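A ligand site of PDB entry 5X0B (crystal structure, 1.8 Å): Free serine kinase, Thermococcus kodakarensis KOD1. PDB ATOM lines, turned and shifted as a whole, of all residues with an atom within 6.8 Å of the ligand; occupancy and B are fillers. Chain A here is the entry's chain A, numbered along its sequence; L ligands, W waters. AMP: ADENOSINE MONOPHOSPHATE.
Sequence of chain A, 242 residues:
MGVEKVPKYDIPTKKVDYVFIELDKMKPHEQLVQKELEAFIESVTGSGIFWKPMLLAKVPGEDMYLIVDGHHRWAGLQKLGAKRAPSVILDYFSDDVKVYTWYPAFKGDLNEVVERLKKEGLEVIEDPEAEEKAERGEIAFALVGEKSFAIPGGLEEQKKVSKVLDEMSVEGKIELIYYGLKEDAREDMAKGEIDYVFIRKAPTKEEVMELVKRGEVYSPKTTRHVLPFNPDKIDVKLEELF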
ATOM      1  N   GLU A  36      13.129   1.013 -11.450  1.00  0.00           N
ATOM      2  CA  GLU A  36      13.357   0.465 -12.789  1.00  0.00           C
ATOM      3  C   GLU A  36      13.564   1.581 -13.814  1.00  0.00           C
ATOM      4  O   GLU A  36      14.415   1.484 -14.680  1.00  0.00           O
ATOM      5  CB  GLU A  36      12.220  -0.471 -13.240  1.00  0.00           C
ATOM      6  CG  GLU A  36      12.077  -1.741 -12.387  1.00  0.00           C
ATOM      7  CD  GLU A  36      10.949  -2.647 -12.838  1.00  0.00           C
ATOM      8  OE1 GLU A  36      10.907  -3.052 -13.991  1.00  0.00           O
ATOM      9  OE2 GLU A  36      10.090  -3.024 -11.999  1.00  0.00           O
ATOM     10  N   LEU A  37      12.772   2.646 -13.695  1.00  0.00           N
ATOM     11  CA  LEU A  37      12.889   3.828 -14.558  1.00  0.00           C
ATOM     12  C   LEU A  37      14.261   4.475 -14.481  1.00  0.00           C
ATOM     13  O   LEU A  37      14.884   4.758 -15.497  1.00  0.00           O
ATOM     14  CB  LEU A  37      11.820   4.837 -14.113  1.00  0.00           C
ATOM     15  CG  LEU A  37      11.682   6.186 -14.814  1.00  0.00           C
ATOM     16  CD1 LEU A  37      11.390   6.019 -16.274  1.00  0.00           C
ATOM     17  CD2 LEU A  37      10.535   6.929 -14.133  1.00  0.00           C
ATOM     18  N   ALA A  39      17.078   3.147 -13.304  1.00  0.00           N
ATOM     19  CA  ALA A  39      18.112   2.238 -13.775  1.00  0.00           C
ATOM     20  C   ALA A  39      18.257   2.242 -15.305  1.00  0.00           C
ATOM     21  O   ALA A  39      19.354   2.318 -15.828  1.00  0.00           O
ATOM     22  CB  ALA A  39      17.845   0.837 -13.261  1.00  0.00           C
ATOM     23  N   PHE A  40      17.124   2.184 -16.018  1.00  0.00           N
ATOM     24  CA  PHE A  40      17.163   2.321 -17.467  1.00  0.00           C
ATOM     25  C   PHE A  40      17.799   3.634 -17.909  1.00  0.00           C
ATOM     26  O   PHE A  40      18.657   3.646 -18.812  1.00  0.00           O
ATOM     27  CB  PHE A  40      15.760   2.171 -18.098  1.00  0.00           C
ATOM     28  CG  PHE A  40      15.747   2.612 -19.518  1.00  0.00           C
ATOM     29  CD1 PHE A  40      16.328   1.800 -20.502  1.00  0.00           C
ATOM     30  CD2 PHE A  40      15.279   3.862 -19.867  1.00  0.00           C
ATOM     31  CE1 PHE A  40      16.404   2.232 -21.800  1.00  0.00           C
ATOM     32  CE2 PHE A  40      15.342   4.304 -21.162  1.00  0.00           C
ATOM     33  CZ  PHE A  40      15.907   3.473 -22.150  1.00  0.00           C
ATOM     34  N   SER A  43      21.465   3.448 -17.510  1.00  0.00           N
ATOM     35  CA  SER A  43      22.088   2.522 -18.450  1.00  0.00           C
ATOM     36  C   SER A  43      22.188   3.080 -19.881  1.00  0.00           C
ATOM     37  O   SER A  43      23.239   2.949 -20.525  1.00  0.00           O
ATOM     38  CB  SER A  43      21.276   1.213 -18.502  1.00  0.00           C
ATOM     39  OG  SER A  43      21.828   0.302 -19.441  1.00  0.00           O
ATOM     40  N   VAL A  44      21.098   3.648 -20.364  1.00  0.00           N
ATOM     41  CA  VAL A  44      21.041   4.067 -21.761  1.00  0.00           C
ATOM     42  C   VAL A  44      21.916   5.294 -21.989  1.00  0.00           C
ATOM     43  O   VAL A  44      22.582   5.382 -23.013  1.00  0.00           O
ATOM     44  CB  VAL A  44      19.580   4.266 -22.275  1.00  0.00           C
ATOM     45  CG1 VAL A  44      18.910   5.554 -21.764  1.00  0.00           C
ATOM     46  CG2 VAL A  44      19.554   4.246 -23.786  1.00  0.00           C
ATOM     47  N   THR A  45      21.923   6.208 -21.027  1.00  0.00           N
ATOM     48  CA  THR A  45      22.771   7.383 -21.086  1.00  0.00           C
ATOM     49  C   THR A  45      24.223   6.958 -20.976  1.00  0.00           C
ATOM     50  O   THR A  45      25.111   7.627 -21.542  1.00  0.00           O
ATOM     51  CB  THR A  45      22.385   8.476 -20.079  1.00  0.00           C
ATOM     52  OG1 THR A  45      22.424   7.985 -18.724  1.00  0.00           O
ATOM     53  CG2 THR A  45      20.999   9.013 -20.367  1.00  0.00           C
ATOM     54  N   SER A  47      25.746   4.082 -22.138  1.00  0.00           N
ATOM     55  CA  SER A  47      26.317   3.510 -23.363  1.00  0.00           C
ATOM     56  C   SER A  47      25.948   4.298 -24.619  1.00  0.00           C
ATOM     57  O   SER A  47      26.663   4.264 -25.607  1.00  0.00           O
ATOM     58  CB  SER A  47      25.894   2.063 -23.503  1.00  0.00           C
ATOM     59  OG  SER A  47      24.541   1.982 -23.824  1.00  0.00           O
ATOM     60  N   GLY A  48      24.843   4.998 -24.572  1.00  0.00           N
ATOM     61  CA  GLY A  48      24.315   5.648 -25.751  1.00  0.00           C
ATOM     62  C   GLY A  48      23.796   4.691 -26.808  1.00  0.00           C
ATOM     63  O   GLY A  48      23.559   5.138 -27.924  1.00  0.00           O
ATOM     64  N   ILE A  49      23.575   3.413 -26.463  1.00  0.00           N
ATOM     65  CA  ILE A  49      23.008   2.397 -27.360  1.00  0.00           C
ATOM     66  C   ILE A  49      21.700   1.920 -26.761  1.00  0.00           C
ATOM     67  O   ILE A  49      21.633   1.617 -25.554  1.00  0.00           O
ATOM     68  CB  ILE A  49      23.945   1.159 -27.479  1.00  0.00           C
ATOM     69  CG1 ILE A  49      25.291   1.569 -28.061  1.00  0.00           C
ATOM     70  CG2 ILE A  49      23.255   0.039 -28.270  1.00  0.00           C
ATOM     71  CD1 ILE A  49      25.218   2.205 -29.417  1.00  0.00           C
ATOM     72  N   PHE A  50      20.666   1.838 -27.592  1.00  0.00           N
ATOM     73  CA  PHE A  50      19.384   1.270 -27.212  1.00  0.00           C
ATOM     74  C   PHE A  50      19.246  -0.072 -27.929  1.00  0.00           C
ATOM     75  O   PHE A  50      19.044  -0.097 -29.099  1.00  0.00           O
ATOM     76  CB  PHE A  50      18.254   2.250 -27.594  1.00  0.00           C
ATOM     77  CG  PHE A  50      16.895   1.834 -27.086  1.00  0.00           C
ATOM     78  CD1 PHE A  50      16.131   0.902 -27.771  1.00  0.00           C
ATOM     79  CD2 PHE A  50      16.374   2.402 -25.910  1.00  0.00           C
ATOM     80  CE1 PHE A  50      14.888   0.534 -27.279  1.00  0.00           C
ATOM     81  CE2 PHE A  50      15.144   2.021 -25.406  1.00  0.00           C
ATOM     82  CZ  PHE A  50      14.387   1.079 -26.100  1.00  0.00           C
ATOM     83  N   TRP A  51      19.385  -1.163 -27.192  1.00  0.00           N
ATOM     84  CA  TRP A  51      19.580  -2.480 -27.772  1.00  0.00           C
ATOM     85  C   TRP A  51      18.418  -3.461 -27.670  1.00  0.00           C
ATOM     86  O   TRP A  51      18.533  -4.579 -28.251  1.00  0.00           O
ATOM     87  CB  TRP A  51      20.850  -3.105 -27.209  1.00  0.00           C
ATOM     88  CG  TRP A  51      20.986  -3.046 -25.724  1.00  0.00           C
ATOM     89  CD1 TRP A  51      21.738  -2.175 -25.030  1.00  0.00           C
ATOM     90  CD2 TRP A  51      20.343  -3.889 -24.760  1.00  0.00           C
ATOM     91  NE1 TRP A  51      21.631  -2.421 -23.683  1.00  0.00           N
ATOM     92  CE2 TRP A  51      20.782  -3.469 -23.492  1.00  0.00           C
ATOM     93  CE3 TRP A  51      19.494  -4.996 -24.839  1.00  0.00           C
ATOM     94  CZ2 TRP A  51      20.362  -4.084 -22.304  1.00  0.00           C
ATOM     95  CZ3 TRP A  51      19.088  -5.624 -23.639  1.00  0.00           C
ATOM     96  CH2 TRP A  51      19.510  -5.147 -22.396  1.00  0.00           C
ATOM     97  N   LYS A  52      17.313  -3.065 -27.005  1.00  0.00           N
ATOM     98  CA  LYS A  52      16.196  -3.930 -26.620  1.00  0.00           C
ATOM     99  C   LYS A  52      14.883  -3.298 -27.097  1.00  0.00           C
ATOM    100  O   LYS A  52      14.323  -2.459 -26.411  1.00  0.00           O
ATOM    101  CB  LYS A  52      16.152  -4.132 -25.097  1.00  0.00           C
ATOM    102  CG  LYS A  52      15.296  -5.326 -24.625  1.00  0.00           C
ATOM    103  CD  LYS A  52      15.297  -5.377 -23.107  1.00  0.00           C
ATOM    104  CE  LYS A  52      14.404  -6.490 -22.620  1.00  0.00           C
ATOM    105  NZ  LYS A  52      14.637  -6.695 -21.168  1.00  0.00           N
ATOM    106  N   PRO A  53      14.360  -3.690 -28.276  1.00  0.00           N
ATOM    107  CA  PRO A  53      13.151  -2.974 -28.748  1.00  0.00           C
ATOM    108  C   PRO A  53      11.936  -3.130 -27.832  1.00  0.00           C
ATOM    109  O   PRO A  53      11.797  -4.151 -27.162  1.00  0.00           O
ATOM    110  CB  PRO A  53      12.840  -3.640 -30.103  1.00  0.00           C
ATOM    111  CG  PRO A  53      13.485  -4.962 -30.016  1.00  0.00           C
ATOM    112  CD  PRO A  53      14.731  -4.778 -29.196  1.00  0.00           C
ATOM    113  N   MET A  54      11.058  -2.138 -27.888  1.00  0.00           N
ATOM    114  CA  MET A  54       9.734  -2.184 -27.293  1.00  0.00           C
ATOM    115  C   MET A  54       8.977  -3.339 -27.941  1.00  0.00           C
ATOM    116  O   MET A  54       9.218  -3.637 -29.102  1.00  0.00           O
ATOM    117  CB  MET A  54       8.963  -0.919 -27.626  1.00  0.00           C
ATOM    118  CG  MET A  54       9.540   0.383 -27.105  1.00  0.00           C
ATOM    119  SD  MET A  54       9.528   0.532 -25.297  1.00  0.00           S
ATOM    120  CE  MET A  54       7.758   0.423 -24.979  1.00  0.00           C
ATOM    121  N   ASP A  69       5.723  -4.945 -23.567  1.00  0.00           N
ATOM    122  CA  ASP A  69       6.969  -4.995 -22.806  1.00  0.00           C
ATOM    123  C   ASP A  69       7.735  -3.732 -23.132  1.00  0.00           C
ATOM    124  O   ASP A  69       7.833  -3.368 -24.298  1.00  0.00           O
ATOM    125  CB  ASP A  69       7.775  -6.241 -23.154  1.00  0.00           C
ATOM    126  CG  ASP A  69       8.973  -6.442 -22.230  1.00  0.00           C
ATOM    127  OD1 ASP A  69       8.761  -6.461 -21.022  1.00  0.00           O
ATOM    128  OD2 ASP A  69      10.121  -6.554 -22.695  1.00  0.00           O
ATOM    129  N   GLY A  70       8.195  -3.036 -22.083  1.00  0.00           N
ATOM    130  CA  GLY A  70       8.935  -1.786 -22.232  1.00  0.00           C
ATOM    131  C   GLY A  70       8.455  -0.566 -21.483  1.00  0.00           C
ATOM    132  O   GLY A  70       8.773   0.546 -21.894  1.00  0.00           O
ATOM    133  N   HIS A  71       7.684  -0.729 -20.406  1.00  0.00           N
ATOM    134  CA  HIS A  71       7.214   0.438 -19.653  1.00  0.00           C
ATOM    135  C   HIS A  71       8.298   1.435 -19.235  1.00  0.00           C
ATOM    136  O   HIS A  71       8.136   2.635 -19.426  1.00  0.00           O
ATOM    137  CB  HIS A  71       6.444   0.009 -18.417  1.00  0.00           C
ATOM    138  CG  HIS A  71       5.146  -0.649 -18.725  1.00  0.00           C
ATOM    139  ND1 HIS A  71       4.798  -1.883 -18.203  1.00  0.00           N
ATOM    140  CD2 HIS A  71       4.099  -0.262 -19.494  1.00  0.00           C
ATOM    141  CE1 HIS A  71       3.586  -2.217 -18.626  1.00  0.00           C
ATOM    142  NE2 HIS A  71       3.142  -1.252 -19.410  1.00  0.00           N
ATOM    143  N   HIS A  72       9.406   0.933 -18.681  1.00  0.00           N
ATOM    144  CA  HIS A  72      10.446   1.826 -18.191  1.00  0.00           C
ATOM    145  C   HIS A  72      11.364   2.389 -19.267  1.00  0.00           C
ATOM    146  O   HIS A  72      11.795   3.525 -19.158  1.00  0.00           O
ATOM    147  CB  HIS A  72      11.189   1.198 -17.031  1.00  0.00           C
ATOM    148  CG  HIS A  72      10.247   0.808 -15.944  1.00  0.00           C
ATOM    149  ND1 HIS A  72       9.575  -0.398 -15.937  1.00  0.00           N
ATOM    150  CD2 HIS A  72       9.758   1.513 -14.907  1.00  0.00           C
ATOM    151  CE1 HIS A  72       8.755  -0.447 -14.910  1.00  0.00           C
ATOM    152  NE2 HIS A  72       8.846   0.708 -14.267  1.00  0.00           N
ATOM    153  N   ARG A  73      11.601   1.622 -20.331  1.00  0.00           N
ATOM    154  CA  ARG A  73      12.215   2.176 -21.525  1.00  0.00           C
ATOM    155  C   ARG A  73      11.398   3.340 -22.065  1.00  0.00           C
ATOM    156  O   ARG A  73      11.929   4.391 -22.330  1.00  0.00           O
ATOM    157  CB  ARG A  73      12.357   1.116 -22.626  1.00  0.00           C
ATOM    158  CG  ARG A  73      13.520   0.184 -22.392  1.00  0.00           C
ATOM    159  CD  ARG A  73      13.410  -1.088 -23.217  1.00  0.00           C
ATOM    160  NE  ARG A  73      12.599  -2.082 -22.525  1.00  0.00           N
ATOM    161  CZ  ARG A  73      12.140  -3.203 -23.071  1.00  0.00           C
ATOM    162  NH1 ARG A  73      12.424  -3.505 -24.332  1.00  0.00           N
ATOM    163  NH2 ARG A  73      11.422  -4.049 -22.333  1.00  0.00           N
ATOM    164  N   TRP A  74      10.090   3.119 -22.253  1.00  0.00           N
ATOM    165  CA  TRP A  74       9.188   4.196 -22.733  1.00  0.00           C
ATOM    166  C   TRP A  74       9.236   5.413 -21.819  1.00  0.00           C
ATOM    167  O   TRP A  74       9.493   6.555 -22.261  1.00  0.00           O
ATOM    168  CB  TRP A  74       7.765   3.646 -22.821  1.00  0.00           C
ATOM    169  CG  TRP A  74       6.699   4.656 -23.016  1.00  0.00           C
ATOM    170  CD1 TRP A  74       6.377   5.326 -24.150  1.00  0.00           C
ATOM    171  CD2 TRP A  74       5.776   5.100 -22.020  1.00  0.00           C
ATOM    172  NE1 TRP A  74       5.293   6.172 -23.916  1.00  0.00           N
ATOM    173  CE2 TRP A  74       4.902   6.035 -22.620  1.00  0.00           C
ATOM    174  CE3 TRP A  74       5.591   4.765 -20.664  1.00  0.00           C
ATOM    175  CZ2 TRP A  74       3.867   6.643 -21.912  1.00  0.00           C
ATOM    176  CZ3 TRP A  74       4.578   5.383 -19.960  1.00  0.00           C
ATOM    177  CH2 TRP A  74       3.733   6.319 -20.574  1.00  0.00           C
HETATM  178  P   AMP L   1      11.241  -2.272 -18.983  1.00  0.00           P
HETATM  179  O1P AMP L   1      11.347  -1.211 -20.064  1.00  0.00           O
HETATM  180  O2P AMP L   1      11.435  -3.684 -19.445  1.00  0.00           O
HETATM  181  O3P AMP L   1      10.038  -2.132 -18.074  1.00  0.00           O
HETATM  182  O5' AMP L   1      12.461  -1.997 -17.944  1.00  0.00           O
HETATM  183  C5' AMP L   1      13.657  -1.335 -18.359  1.00  0.00           C
HETATM  184  C4' AMP L   1      14.404  -2.205 -19.363  1.00  0.00           C
HETATM  185  O4' AMP L   1      15.500  -1.503 -19.953  1.00  0.00           O
HETATM  186  C3' AMP L   1      15.016  -3.472 -18.762  1.00  0.00           C
HETATM  187  O3' AMP L   1      14.286  -4.609 -19.248  1.00  0.00           O
HETATM  188  C2' AMP L   1      16.446  -3.513 -19.256  1.00  0.00           C
HETATM  189  O2' AMP L   1      16.820  -4.789 -19.788  1.00  0.00           O
HETATM  190  C1' AMP L   1      16.392  -2.514 -20.383  1.00  0.00           C
HETATM  191  N9  AMP L   1      17.632  -1.819 -20.718  1.00  0.00           N
HETATM  192  C8  AMP L   1      18.701  -1.528 -19.926  1.00  0.00           C
HETATM  193  N7  AMP L   1      19.600  -0.824 -20.622  1.00  0.00           N
HETATM  194  C5  AMP L   1      19.101  -0.631 -21.874  1.00  0.00           C
HETATM  195  C6  AMP L   1      19.545   0.030 -23.102  1.00  0.00           C
HETATM  196  N6  AMP L   1      20.761   0.647 -23.136  1.00  0.00           N
HETATM  197  N1  AMP L   1      18.716  -0.016 -24.179  1.00  0.00           N
HETATM  198  C2  AMP L   1      17.513  -0.644 -24.147  1.00  0.00           C
HETATM  199  N3  AMP L   1      17.052  -1.269 -23.049  1.00  0.00           N
HETATM  200  C4  AMP L   1      17.798  -1.298 -21.924  1.00  0.00           C
HETATM  201  O   HOH W   1      18.173  -1.210 -16.680  1.00  0.00           O
HETATM  202  O   HOH W   2      12.836  -3.165 -15.472  1.00  0.00           O
HETATM  203  O   HOH W   3       7.691  -3.353 -19.306  1.00  0.00           O
HETATM  204  O   HOH W   4      10.096  -5.822 -18.642  1.00  0.00           O
HETATM  205  O   HOH W   5       8.850  -3.730 -16.162  1.00  0.00           O
HETATM  206  O   HOH W   6      15.519  -0.959 -15.424  1.00  0.00           O
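Phe 40 touches the ligand. Val 44 touches the ligand. Phe 50 touches the ligand. C of Gly 70 touches O1P of the ligand (3.3 Å). His 71 touches the ligand (N to O3P, 3.6 Å). Hydrophobic or aromatic side chains within 4 Å of the ligand: Phe 40, Val 44, Phe 50, Trp 51 and His 72.
Water W4 bridges O2P of the ligand and OD1 of Asp 69. Water W2 lies within hydrogen-bond range of OE1 of Glu 36 (2.4 Å) and O5' of the ligand (2.8 Å). Water W5 lies within hydrogen-bond range of an oxygen (O3P) of the ligand, the side-chain carboxylate of Glu 36 and a ring nitrogen (ND1) of His 72. Water W3 lies within hydrogen-bond range of N of Gly 70, N of His 71 and O3P of the ligand.
N6 of the ligand lies within hydrogen-bond range of O of Ile 49 (2.7 Å). OG of Ser 43 is in hydrogen-bond range of N7 of the ligand, at 2.8 Å. N of His 72 sits at hydrogen-bond distance from O3P of the ligand (3.2 Å). A ring nitrogen (ND1) of His 72 lies within hydrogen-bond range of an oxygen (O3P) of the ligand, at 2.8 Å. An oxygen (O1P) of the ligand sits at hydrogen-bond distance from the backbone NH of Arg 73 (2.9 Å). The guanidinium group (NE) of Arg 73 lies within salt-bridge range of an oxygen (O1P) of the ligand (2.9 Å). The side-chain amino group (NZ) of Lys 52 lies within hydrogen-bond range of an oxygen (O3') of the ligand (2.9 Å). N of Trp 51 lies within hydrogen-bond range of N1 of the ligand (3.3 Å).
The backbone NH (N) of Ile 49 sits close to the side-chain hydroxyl (OG) of Ser 47 (3.2 Å). The backbone carbonyl oxygen (O) of Lys 52 is in hydrogen-bond range of the guanidinium group (NH1) of Arg 73, 3.0 Å away. NH2 of Arg 73 is in salt-bridge range of OD2 of Asp 69, at 2.8 Å. O of Pro 53 sits at hydrogen-bond distance from NH1 of Arg 73 (3.0 Å).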
